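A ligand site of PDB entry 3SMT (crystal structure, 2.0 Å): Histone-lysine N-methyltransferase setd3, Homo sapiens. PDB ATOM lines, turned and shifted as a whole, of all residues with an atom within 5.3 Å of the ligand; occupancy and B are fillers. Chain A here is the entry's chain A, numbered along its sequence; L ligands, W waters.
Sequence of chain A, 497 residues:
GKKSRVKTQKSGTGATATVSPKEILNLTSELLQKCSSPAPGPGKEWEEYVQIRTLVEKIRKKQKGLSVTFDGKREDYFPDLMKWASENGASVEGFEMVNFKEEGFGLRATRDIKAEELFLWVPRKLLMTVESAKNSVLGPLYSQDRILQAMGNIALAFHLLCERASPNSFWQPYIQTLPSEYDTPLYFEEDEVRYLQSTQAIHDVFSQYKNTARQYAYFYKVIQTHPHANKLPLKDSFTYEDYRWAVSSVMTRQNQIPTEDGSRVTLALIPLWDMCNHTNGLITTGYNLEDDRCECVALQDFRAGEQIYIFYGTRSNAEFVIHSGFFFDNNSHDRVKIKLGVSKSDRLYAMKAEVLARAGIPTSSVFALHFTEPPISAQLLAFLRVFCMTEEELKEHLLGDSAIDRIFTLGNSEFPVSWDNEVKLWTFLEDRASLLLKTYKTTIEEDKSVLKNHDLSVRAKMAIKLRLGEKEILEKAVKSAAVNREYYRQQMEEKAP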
ATOM      1  N   ARG A  74     -20.475 -41.149  20.413  1.00  0.00           N
ATOM      2  CA  ARG A  74     -20.733 -39.855  19.746  1.00  0.00           C
ATOM      3  C   ARG A  74     -19.491 -39.266  19.053  1.00  0.00           C
ATOM      4  O   ARG A  74     -19.645 -38.781  17.943  1.00  0.00           O
ATOM      5  CB  ARG A  74     -21.426 -38.815  20.656  1.00  0.00           C
ATOM      6  CG  ARG A  74     -20.619 -38.276  21.845  1.00  0.00           C
ATOM      7  CD  ARG A  74     -21.458 -37.416  22.770  1.00  0.00           C
ATOM      8  NE  ARG A  74     -21.898 -36.160  22.141  1.00  0.00           N
ATOM      9  CZ  ARG A  74     -21.953 -34.990  22.774  1.00  0.00           C
ATOM     10  NH1 ARG A  74     -21.548 -34.893  24.037  1.00  0.00           N
ATOM     11  NH2 ARG A  74     -22.339 -33.899  22.125  1.00  0.00           N
ATOM     12  N   GLU A 102     -14.156 -30.474  32.670  1.00  0.00           N
ATOM     13  CA  GLU A 102     -15.259 -29.863  33.409  1.00  0.00           C
ATOM     14  C   GLU A 102     -16.620 -29.750  32.646  1.00  0.00           C
ATOM     15  O   GLU A 102     -17.659 -29.849  33.278  1.00  0.00           O
ATOM     16  CB  GLU A 102     -14.847 -28.494  33.973  1.00  0.00           C
ATOM     17  CG  GLU A 102     -13.634 -28.551  34.903  1.00  0.00           C
ATOM     18  CD  GLU A 102     -13.792 -29.412  36.138  1.00  0.00           C
ATOM     19  N   GLU A 103     -16.622 -29.518  31.326  1.00  0.00           N
ATOM     20  CA  GLU A 103     -17.879 -29.250  30.624  1.00  0.00           C
ATOM     21  C   GLU A 103     -18.360 -30.323  29.675  1.00  0.00           C
ATOM     22  O   GLU A 103     -19.428 -30.186  29.073  1.00  0.00           O
ATOM     23  CB  GLU A 103     -17.732 -27.927  29.850  1.00  0.00           C
ATOM     24  CG  GLU A 103     -17.203 -26.743  30.660  1.00  0.00           C
ATOM     25  CD  GLU A 103     -15.708 -26.469  30.663  1.00  0.00           C
ATOM     26  OE1 GLU A 103     -14.913 -27.317  30.217  1.00  0.00           O
ATOM     27  OE2 GLU A 103     -15.340 -25.389  31.163  1.00  0.00           O
ATOM     28  N   GLY A 104     -17.595 -31.388  29.539  1.00  0.00           N
ATOM     29  CA  GLY A 104     -17.897 -32.459  28.587  1.00  0.00           C
ATOM     30  C   GLY A 104     -17.391 -32.016  27.231  1.00  0.00           C
ATOM     31  O   GLY A 104     -16.483 -31.202  27.178  1.00  0.00           O
ATOM     32  N   PHE A 105     -18.033 -32.463  26.132  1.00  0.00           N
ATOM     33  CA  PHE A 105     -17.586 -32.106  24.776  1.00  0.00           C
ATOM     34  C   PHE A 105     -17.831 -30.641  24.463  1.00  0.00           C
ATOM     35  O   PHE A 105     -18.768 -30.015  24.974  1.00  0.00           O
ATOM     36  CB  PHE A 105     -18.165 -33.056  23.684  1.00  0.00           C
ATOM     37  CG  PHE A 105     -17.475 -34.409  23.591  1.00  0.00           C
ATOM     38  CD1 PHE A 105     -16.298 -34.559  22.870  1.00  0.00           C
ATOM     39  CD2 PHE A 105     -18.014 -35.524  24.222  1.00  0.00           C
ATOM     40  CE1 PHE A 105     -15.655 -35.805  22.792  1.00  0.00           C
ATOM     41  CE2 PHE A 105     -17.376 -36.786  24.147  1.00  0.00           C
ATOM     42  CZ  PHE A 105     -16.206 -36.915  23.430  1.00  0.00           C
ATOM     43  N   GLY A 106     -16.914 -30.063  23.708  1.00  0.00           N
ATOM     44  CA  GLY A 106     -16.931 -28.667  23.342  1.00  0.00           C
ATOM     45  C   GLY A 106     -16.000 -28.385  22.186  1.00  0.00           C
ATOM     46  O   GLY A 106     -15.430 -29.314  21.613  1.00  0.00           O
ATOM     47  N   THR A 177     -24.420 -37.088  16.918  1.00  0.00           N
ATOM     48  CA  THR A 177     -23.369 -36.462  17.746  1.00  0.00           C
ATOM     49  C   THR A 177     -23.937 -35.879  19.048  1.00  0.00           C
ATOM     50  O   THR A 177     -23.181 -35.290  19.824  1.00  0.00           O
ATOM     51  CB  THR A 177     -22.577 -35.396  16.959  1.00  0.00           C
ATOM     52  OG1 THR A 177     -23.497 -34.403  16.480  1.00  0.00           O
ATOM     53  CG2 THR A 177     -21.825 -35.981  15.796  1.00  0.00           C
ATOM     54  N   PRO A 179     -25.605 -35.934  22.926  1.00  0.00           N
ATOM     55  CA  PRO A 179     -25.398 -36.847  24.082  1.00  0.00           C
ATOM     56  C   PRO A 179     -26.526 -37.885  24.158  1.00  0.00           C
ATOM     57  O   PRO A 179     -27.625 -37.632  23.662  1.00  0.00           O
ATOM     58  CB  PRO A 179     -25.445 -35.909  25.291  1.00  0.00           C
ATOM     59  CG  PRO A 179     -25.195 -34.540  24.737  1.00  0.00           C
ATOM     60  CD  PRO A 179     -25.760 -34.535  23.356  1.00  0.00           C
ATOM     61  N   TYR A 182     -28.291 -36.835  29.966  1.00  0.00           N
ATOM     62  CA  TYR A 182     -28.012 -35.490  30.480  1.00  0.00           C
ATOM     63  C   TYR A 182     -27.987 -35.499  31.988  1.00  0.00           C
ATOM     64  O   TYR A 182     -28.340 -36.520  32.594  1.00  0.00           O
ATOM     65  CB  TYR A 182     -29.104 -34.525  29.959  1.00  0.00           C
ATOM     66  CG  TYR A 182     -29.127 -34.448  28.455  1.00  0.00           C
ATOM     67  CD1 TYR A 182     -28.220 -33.639  27.766  1.00  0.00           C
ATOM     68  CD2 TYR A 182     -29.987 -35.247  27.697  1.00  0.00           C
ATOM     69  CE1 TYR A 182     -28.227 -33.572  26.384  1.00  0.00           C
ATOM     70  CE2 TYR A 182     -29.931 -35.261  26.311  1.00  0.00           C
ATOM     71  CZ  TYR A 182     -29.068 -34.391  25.658  1.00  0.00           C
ATOM     72  OH  TYR A 182     -29.040 -34.307  24.294  1.00  0.00           O
ATOM     73  N   THR A 252     -31.615 -28.270  27.264  1.00  0.00           N
ATOM     74  CA  THR A 252     -30.192 -28.012  27.507  1.00  0.00           C
ATOM     75  C   THR A 252     -29.537 -27.339  26.315  1.00  0.00           C
ATOM     76  O   THR A 252     -28.408 -26.867  26.435  1.00  0.00           O
ATOM     77  CB  THR A 252     -29.377 -29.312  27.847  1.00  0.00           C
ATOM     78  OG1 THR A 252     -29.387 -30.207  26.733  1.00  0.00           O
ATOM     79  CG2 THR A 252     -29.888 -30.029  29.106  1.00  0.00           C
ATOM     80  N   ARG A 253     -30.192 -27.367  25.141  1.00  0.00           N
ATOM     81  CA  ARG A 253     -29.563 -26.888  23.900  1.00  0.00           C
ATOM     82  C   ARG A 253     -30.327 -25.837  23.101  1.00  0.00           C
ATOM     83  O   ARG A 253     -29.729 -25.224  22.205  1.00  0.00           O
ATOM     84  CB  ARG A 253     -29.272 -28.083  22.993  1.00  0.00           C
ATOM     85  CG  ARG A 253     -28.462 -29.176  23.689  1.00  0.00           C
ATOM     86  CD  ARG A 253     -28.197 -30.338  22.793  1.00  0.00           C
ATOM     87  NE  ARG A 253     -27.018 -30.168  21.940  1.00  0.00           N
ATOM     88  CZ  ARG A 253     -25.788 -30.584  22.250  1.00  0.00           C
ATOM     89  NH1 ARG A 253     -24.805 -30.458  21.372  1.00  0.00           N
ATOM     90  NH2 ARG A 253     -25.538 -31.082  23.459  1.00  0.00           N
ATOM     91  N   ASP A 274     -24.174 -25.433  18.966  1.00  0.00           N
ATOM     92  CA  ASP A 274     -24.587 -25.907  20.295  1.00  0.00           C
ATOM     93  C   ASP A 274     -23.572 -26.855  20.937  1.00  0.00           C
ATOM     94  O   ASP A 274     -23.819 -27.326  22.047  1.00  0.00           O
ATOM     95  CB  ASP A 274     -26.014 -26.459  20.309  1.00  0.00           C
ATOM     96  CG  ASP A 274     -26.224 -27.849  19.721  1.00  0.00           C
ATOM     97  OD1 ASP A 274     -25.228 -28.460  19.257  1.00  0.00           O
ATOM     98  OD2 ASP A 274     -27.390 -28.320  19.731  1.00  0.00           O
ATOM     99  N   MET A 275     -22.407 -27.083  20.277  1.00  0.00           N
ATOM    100  CA  MET A 275     -21.273 -27.785  20.888  1.00  0.00           C
ATOM    101  C   MET A 275     -20.542 -26.829  21.869  1.00  0.00           C
ATOM    102  O   MET A 275     -19.795 -27.308  22.720  1.00  0.00           O
ATOM    103  CB  MET A 275     -20.283 -28.305  19.853  1.00  0.00           C
ATOM    104  CG  MET A 275     -20.800 -29.477  19.056  1.00  0.00           C
ATOM    105  SD  MET A 275     -21.450 -30.960  20.136  1.00  0.00           S
ATOM    106  CE  MET A 275     -19.840 -31.356  21.155  1.00  0.00           C
ATOM    107  N   CYS A 276     -20.790 -25.489  21.810  1.00  0.00           N
ATOM    108  CA  CYS A 276     -20.114 -24.528  22.677  1.00  0.00           C
ATOM    109  C   CYS A 276     -20.624 -24.555  24.079  1.00  0.00           C
ATOM    110  O   CYS A 276     -21.829 -24.386  24.312  1.00  0.00           O
ATOM    111  CB  CYS A 276     -20.185 -23.109  22.116  1.00  0.00           C
ATOM    112  SG  CYS A 276     -19.397 -22.896  20.508  1.00  0.00           S
ATOM    113  N   ASN A 277     -19.675 -24.640  25.034  1.00  0.00           N
ATOM    114  CA  ASN A 277     -20.015 -24.593  26.457  1.00  0.00           C
ATOM    115  C   ASN A 277     -20.131 -23.147  26.908  1.00  0.00           C
ATOM    116  O   ASN A 277     -19.869 -22.235  26.127  1.00  0.00           O
ATOM    117  CB  ASN A 277     -19.019 -25.403  27.286  1.00  0.00           C
ATOM    118  CG  ASN A 277     -19.170 -26.866  26.965  1.00  0.00           C
ATOM    119  OD1 ASN A 277     -20.292 -27.405  26.977  1.00  0.00           O
ATOM    120  ND2 ASN A 277     -18.065 -27.520  26.598  1.00  0.00           N
ATOM    121  N   HIS A 278     -20.635 -22.948  28.128  1.00  0.00           N
ATOM    122  CA  HIS A 278     -20.861 -21.625  28.721  1.00  0.00           C
ATOM    123  C   HIS A 278     -19.685 -21.169  29.549  1.00  0.00           C
ATOM    124  O   HIS A 278     -19.105 -21.949  30.298  1.00  0.00           O
ATOM    125  CB  HIS A 278     -22.095 -21.687  29.660  1.00  0.00           C
ATOM    126  CG  HIS A 278     -22.309 -20.439  30.499  1.00  0.00           C
ATOM    127  ND1 HIS A 278     -22.970 -19.332  29.991  1.00  0.00           N
ATOM    128  CD2 HIS A 278     -21.920 -20.161  31.765  1.00  0.00           C
ATOM    129  CE1 HIS A 278     -22.982 -18.433  30.962  1.00  0.00           C
ATOM    130  NE2 HIS A 278     -22.351 -18.873  32.046  1.00  0.00           N
ATOM    131  N   THR A 279     -19.394 -19.865  29.447  1.00  0.00           N
ATOM    132  CA  THR A 279     -18.496 -19.090  30.285  1.00  0.00           C
ATOM    133  C   THR A 279     -18.946 -17.625  30.256  1.00  0.00           C
ATOM    134  O   THR A 279     -19.695 -17.230  29.366  1.00  0.00           O
ATOM    135  CB  THR A 279     -17.005 -19.265  29.925  1.00  0.00           C
ATOM    136  OG1 THR A 279     -16.287 -19.101  31.149  1.00  0.00           O
ATOM    137  CG2 THR A 279     -16.487 -18.233  28.870  1.00  0.00           C
ATOM    138  N   TYR A 309     -16.015 -20.706  24.007  1.00  0.00           N
ATOM    139  CA  TYR A 309     -17.275 -20.725  24.740  1.00  0.00           C
ATOM    140  C   TYR A 309     -18.234 -19.665  24.223  1.00  0.00           C
ATOM    141  O   TYR A 309     -17.814 -18.727  23.563  1.00  0.00           O
ATOM    142  CB  TYR A 309     -17.001 -20.334  26.206  1.00  0.00           C
ATOM    143  CG  TYR A 309     -16.138 -21.262  27.048  1.00  0.00           C
ATOM    144  CD1 TYR A 309     -16.713 -22.259  27.821  1.00  0.00           C
ATOM    145  CD2 TYR A 309     -14.782 -20.985  27.241  1.00  0.00           C
ATOM    146  CE1 TYR A 309     -15.950 -23.030  28.700  1.00  0.00           C
ATOM    147  CE2 TYR A 309     -14.013 -21.738  28.132  1.00  0.00           C
ATOM    148  CZ  TYR A 309     -14.606 -22.754  28.871  1.00  0.00           C
ATOM    149  OH  TYR A 309     -13.905 -23.534  29.768  1.00  0.00           O
ATOM    150  N   TYR A 312     -24.424 -18.194  27.824  1.00  0.00           N
ATOM    151  CA  TYR A 312     -25.799 -18.719  27.718  1.00  0.00           C
ATOM    152  C   TYR A 312     -26.838 -17.698  28.238  1.00  0.00           C
ATOM    153  O   TYR A 312     -28.030 -17.852  27.967  1.00  0.00           O
ATOM    154  CB  TYR A 312     -25.963 -20.058  28.473  1.00  0.00           C
ATOM    155  CG  TYR A 312     -25.295 -21.308  27.894  1.00  0.00           C
ATOM    156  CD1 TYR A 312     -24.367 -21.209  26.850  1.00  0.00           C
ATOM    157  CD2 TYR A 312     -25.522 -22.567  28.460  1.00  0.00           C
ATOM    158  CE1 TYR A 312     -23.737 -22.352  26.343  1.00  0.00           C
ATOM    159  CE2 TYR A 312     -24.880 -23.697  27.980  1.00  0.00           C
ATOM    160  CZ  TYR A 312     -23.994 -23.596  26.908  1.00  0.00           C
ATOM    161  OH  TYR A 312     -23.416 -24.742  26.402  1.00  0.00           O
ATOM    162  N   SER A 324     -30.304 -26.983  32.321  1.00  0.00           N
ATOM    163  CA  SER A 324     -29.087 -27.277  31.527  1.00  0.00           C
ATOM    164  C   SER A 324     -28.243 -28.421  32.108  1.00  0.00           C
ATOM    165  O   SER A 324     -27.285 -28.850  31.490  1.00  0.00           O
ATOM    166  CB  SER A 324     -28.228 -26.027  31.369  1.00  0.00           C
ATOM    167  OG  SER A 324     -28.947 -25.015  30.675  1.00  0.00           O
ATOM    168  N   GLY A 325     -28.574 -28.871  33.310  1.00  0.00           N
ATOM    169  CA  GLY A 325     -27.830 -29.976  33.917  1.00  0.00           C
ATOM    170  C   GLY A 325     -26.420 -29.673  34.390  1.00  0.00           C
ATOM    171  O   GLY A 325     -25.568 -30.574  34.385  1.00  0.00           O
ATOM    172  N   PHE A 326     -26.143 -28.440  34.841  1.00  0.00           N
ATOM    173  CA  PHE A 326     -24.824 -28.126  35.372  1.00  0.00           C
ATOM    174  C   PHE A 326     -24.927 -27.025  36.380  1.00  0.00           C
ATOM    175  O   PHE A 326     -25.881 -26.298  36.369  1.00  0.00           O
ATOM    176  CB  PHE A 326     -23.802 -27.795  34.235  1.00  0.00           C
ATOM    177  CG  PHE A 326     -23.885 -26.421  33.595  1.00  0.00           C
ATOM    178  CD1 PHE A 326     -23.036 -25.404  34.000  1.00  0.00           C
ATOM    179  CD2 PHE A 326     -24.724 -26.187  32.509  1.00  0.00           C
ATOM    180  CE1 PHE A 326     -23.060 -24.150  33.362  1.00  0.00           C
ATOM    181  CE2 PHE A 326     -24.754 -24.937  31.879  1.00  0.00           C
ATOM    182  CZ  PHE A 326     -23.926 -23.932  32.329  1.00  0.00           C
ATOM    183  N   PHE A 327     -23.979 -26.925  37.272  1.00  0.00           N
ATOM    184  CA  PHE A 327     -23.895 -25.871  38.247  1.00  0.00           C
ATOM    185  C   PHE A 327     -22.678 -25.073  37.845  1.00  0.00           C
ATOM    186  O   PHE A 327     -21.586 -25.657  37.704  1.00  0.00           O
ATOM    187  CB  PHE A 327     -23.674 -26.458  39.656  1.00  0.00           C
ATOM    188  CG  PHE A 327     -23.631 -25.422  40.763  1.00  0.00           C
ATOM    189  CD1 PHE A 327     -24.765 -25.106  41.494  1.00  0.00           C
ATOM    190  CD2 PHE A 327     -22.427 -24.810  41.110  1.00  0.00           C
ATOM    191  CE1 PHE A 327     -24.705 -24.203  42.556  1.00  0.00           C
ATOM    192  CE2 PHE A 327     -22.375 -23.890  42.148  1.00  0.00           C
ATOM    193  CZ  PHE A 327     -23.520 -23.574  42.859  1.00  0.00           C
ATOM    194  N   PHE A 328     -22.818 -23.751  37.672  1.00  0.00           N
ATOM    195  CA  PHE A 328     -21.666 -22.924  37.289  1.00  0.00           C
ATOM    196  C   PHE A 328     -21.080 -22.248  38.514  1.00  0.00           C
ATOM    197  O   PHE A 328     -21.700 -21.349  39.078  1.00  0.00           O
ATOM    198  CB  PHE A 328     -22.069 -21.906  36.173  1.00  0.00           C
ATOM    199  CG  PHE A 328     -20.913 -21.217  35.488  1.00  0.00           C
ATOM    200  CD1 PHE A 328     -19.934 -21.945  34.820  1.00  0.00           C
ATOM    201  CD2 PHE A 328     -20.796 -19.832  35.507  1.00  0.00           C
ATOM    202  CE1 PHE A 328     -18.860 -21.302  34.201  1.00  0.00           C
ATOM    203  CE2 PHE A 328     -19.710 -19.191  34.895  1.00  0.00           C
ATOM    204  CZ  PHE A 328     -18.753 -19.933  34.258  1.00  0.00           C
HETATM  205  N1  LIG L   1     -21.048 -30.049  26.362  1.00  0.00           N
HETATM  206  C1  LIG L   1     -22.225 -30.207  25.455  1.00  0.00           C
HETATM  207  C2  LIG L   1     -22.123 -31.489  24.652  1.00  0.00           C
HETATM  208  O1  LIG L   1     -21.272 -32.319  24.909  1.00  0.00           O
HETATM  209  O2  LIG L   1     -22.893 -31.726  23.683  1.00  0.00           O
HETATM  210  C3  LIG L   1     -22.114 -29.009  24.422  1.00  0.00           C
HETATM  211  C4  LIG L   1     -22.785 -27.730  24.946  1.00  0.00           C
HETATM  212  S1  LIG L   1     -24.595 -28.025  25.039  1.00  0.00           S
HETATM  213  C5  LIG L   1     -25.427 -26.534  24.486  1.00  0.00           C
HETATM  214  C6  LIG L   1     -24.928 -27.775  26.812  1.00  0.00           C
HETATM  215  C7  LIG L   1     -24.430 -28.805  27.835  1.00  0.00           C
HETATM  216  O3  LIG L   1     -23.021 -28.607  28.095  1.00  0.00           O
HETATM  217  C8  LIG L   1     -25.057 -28.494  29.199  1.00  0.00           C
HETATM  218  O4  LIG L   1     -26.301 -29.185  29.292  1.00  0.00           O
HETATM  219  C9  LIG L   1     -24.032 -29.118  30.193  1.00  0.00           C
HETATM  220  O5  LIG L   1     -24.097 -30.606  30.153  1.00  0.00           O
HETATM  221  C10 LIG L   1     -22.703 -28.628  29.491  1.00  0.00           C
HETATM  222  N2  LIG L   1     -22.107 -27.358  29.843  1.00  0.00           N
HETATM  223  C11 LIG L   1     -22.067 -26.164  29.134  1.00  0.00           C
HETATM  224  N3  LIG L   1     -21.328 -25.321  29.788  1.00  0.00           N
HETATM  225  C12 LIG L   1     -20.897 -25.887  30.938  1.00  0.00           C
HETATM  226  C13 LIG L   1     -20.108 -25.471  32.075  1.00  0.00           C
HETATM  227  N4  LIG L   1     -19.538 -24.222  32.116  1.00  0.00           N
HETATM  228  N5  LIG L   1     -19.808 -26.399  33.030  1.00  0.00           N
HETATM  229  C14 LIG L   1     -20.270 -27.642  32.964  1.00  0.00           C
HETATM  230  N6  LIG L   1     -21.072 -28.023  31.987  1.00  0.00           N
HETATM  231  C15 LIG L   1     -21.346 -27.200  30.953  1.00  0.00           C
HETATM  232  O   HOH W   1     -21.937 -32.165  27.933  1.00  0.00           O
HETATM  233  O   HOH W   2     -22.065 -30.826  32.030  1.00  0.00           O
HETATM  234  O   HOH W   3     -20.402 -34.482  26.966  1.00  0.00           O
HETATM  235  O   HOH W   4     -26.499 -32.259  31.135  1.00  0.00           O
HETATM  236  O   HOH W   5     -24.007 -33.693  30.861  1.00  0.00           O
HETATM  237  O   HOH W   6     -26.743 -23.822  22.989  1.00  0.00           O
HETATM  238  O   HOH W   7     -18.512 -25.835  35.291  1.00  0.00           O
HETATM  239  O   HOH W   8     -24.995 -32.107  27.740  1.00  0.00           O
HETATM  240  O   HOH W   9     -16.651 -23.763  32.903  1.00  0.00           O
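An oxygen (O4) of the ligand lies within hydrogen-bond range of the backbone carbonyl oxygen (O) of Ser 324 (2.4 Å).
The backbone NH (N) of Phe 105 lies close to an oxygen (O1) of the ligand.
N1 of the ligand lies within hydrogen-bond range of O of Phe 105, 2.7 Å away.
NH2 of Arg 74 lies within salt-bridge range of O2 of the ligand (2.7 Å).
NH2 of Arg 253 is in salt-bridge range of O2 of the ligand (2.7 Å).
OD1 of Asn 277 sits at hydrogen-bond distance from N1 of the ligand (2.8 Å).
The backbone NH (N) of His 278 sits at hydrogen-bond distance from a nitrogen (N3) of the ligand, 3.0 Å away.
The backbone carbonyl oxygen (O) of His 278 is in hydrogen-bond range of a nitrogen (N4) of the ligand, 2.9 Å away.
The backbone carbonyl oxygen (O) of Glu 103 is in hydrogen-bond range of a nitrogen (N1) of the ligand (3.2 Å).
The backbone carbonyl oxygen (O) of Phe 105 is in hydrogen-bond range of the side-chain amide nitrogen (ND2) of Asn 277 (3.1 Å).
The guanidinium group of Arg 74 is in hydrogen-bond range of the side-chain sulfur of Met 275, 3.7 Å away.
NE of Arg 74 is in hydrogen-bond range of O of Thr 177 (2.8 Å).
NE of Arg 253 is in salt-bridge range of OD2 of Asp 274 (2.9 Å).
SD of Met 275 is in hydrogen-bond range of NH1 of Arg 253 (3.6 Å).
ND1 of His 278 lies within hydrogen-bond range of N of Tyr 312 (2.8 Å).
The side-chain carboxylate (OE2) of Glu 103 is in hydrogen-bond range of the side-chain hydroxyl (OH) of Tyr 309 (2.7 Å).
The side-chain hydroxyl (OH) of Tyr 312 lies within hydrogen-bond range of the backbone carbonyl oxygen (O) of Cys 276, at 2.6 Å.
The backbone carbonyl oxygen (O) of Asp 274 lies close to a sulfur (S1) of the ligand, at 3.2 Å.
S1 of the ligand lies close to OH of Tyr 312, at 3.7 Å.
Glu 102 touches the ligand.
Pro 179 touches the ligand (CG to O2, 3.8 Å).
Thr 252 touches the ligand (CB to O4, 3.4 Å).
Met 275 touches the ligand (O to C3, 3.3 Å).
Cys 276 touches the ligand (O to C4, 3.5 Å).
Phe 326 touches the ligand (CE1 to C13, 3.5 Å).
Phe 328 touches the ligand (CD1 to N4, 3.6 Å).
Hydrophobic or aromatic side chains that line the ligand: Phe 105, Pro 179, Met 275, His 278, Tyr 312, Phe 326 and Phe 328.
Of the 24 residues printed, 16 come within 4 Å of the ligand.
Water W1 bridges N1 of the ligand (2.8 Å) and O of Glu 103 (3.4 Å).
Water W9 lies within hydrogen-bond range of the side-chain carboxylate of Glu 103 (2.7 Å) and a nitrogen (N4) of the ligand (3.0 Å).
Water W3 lies within hydrogen-bond range of an oxygen (O1) of the ligand (3.1 Å), the guanidinium group (NH1) of Arg 74 (3.2 Å) and the backbone NH (N) of Phe 105 (3.2 Å).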
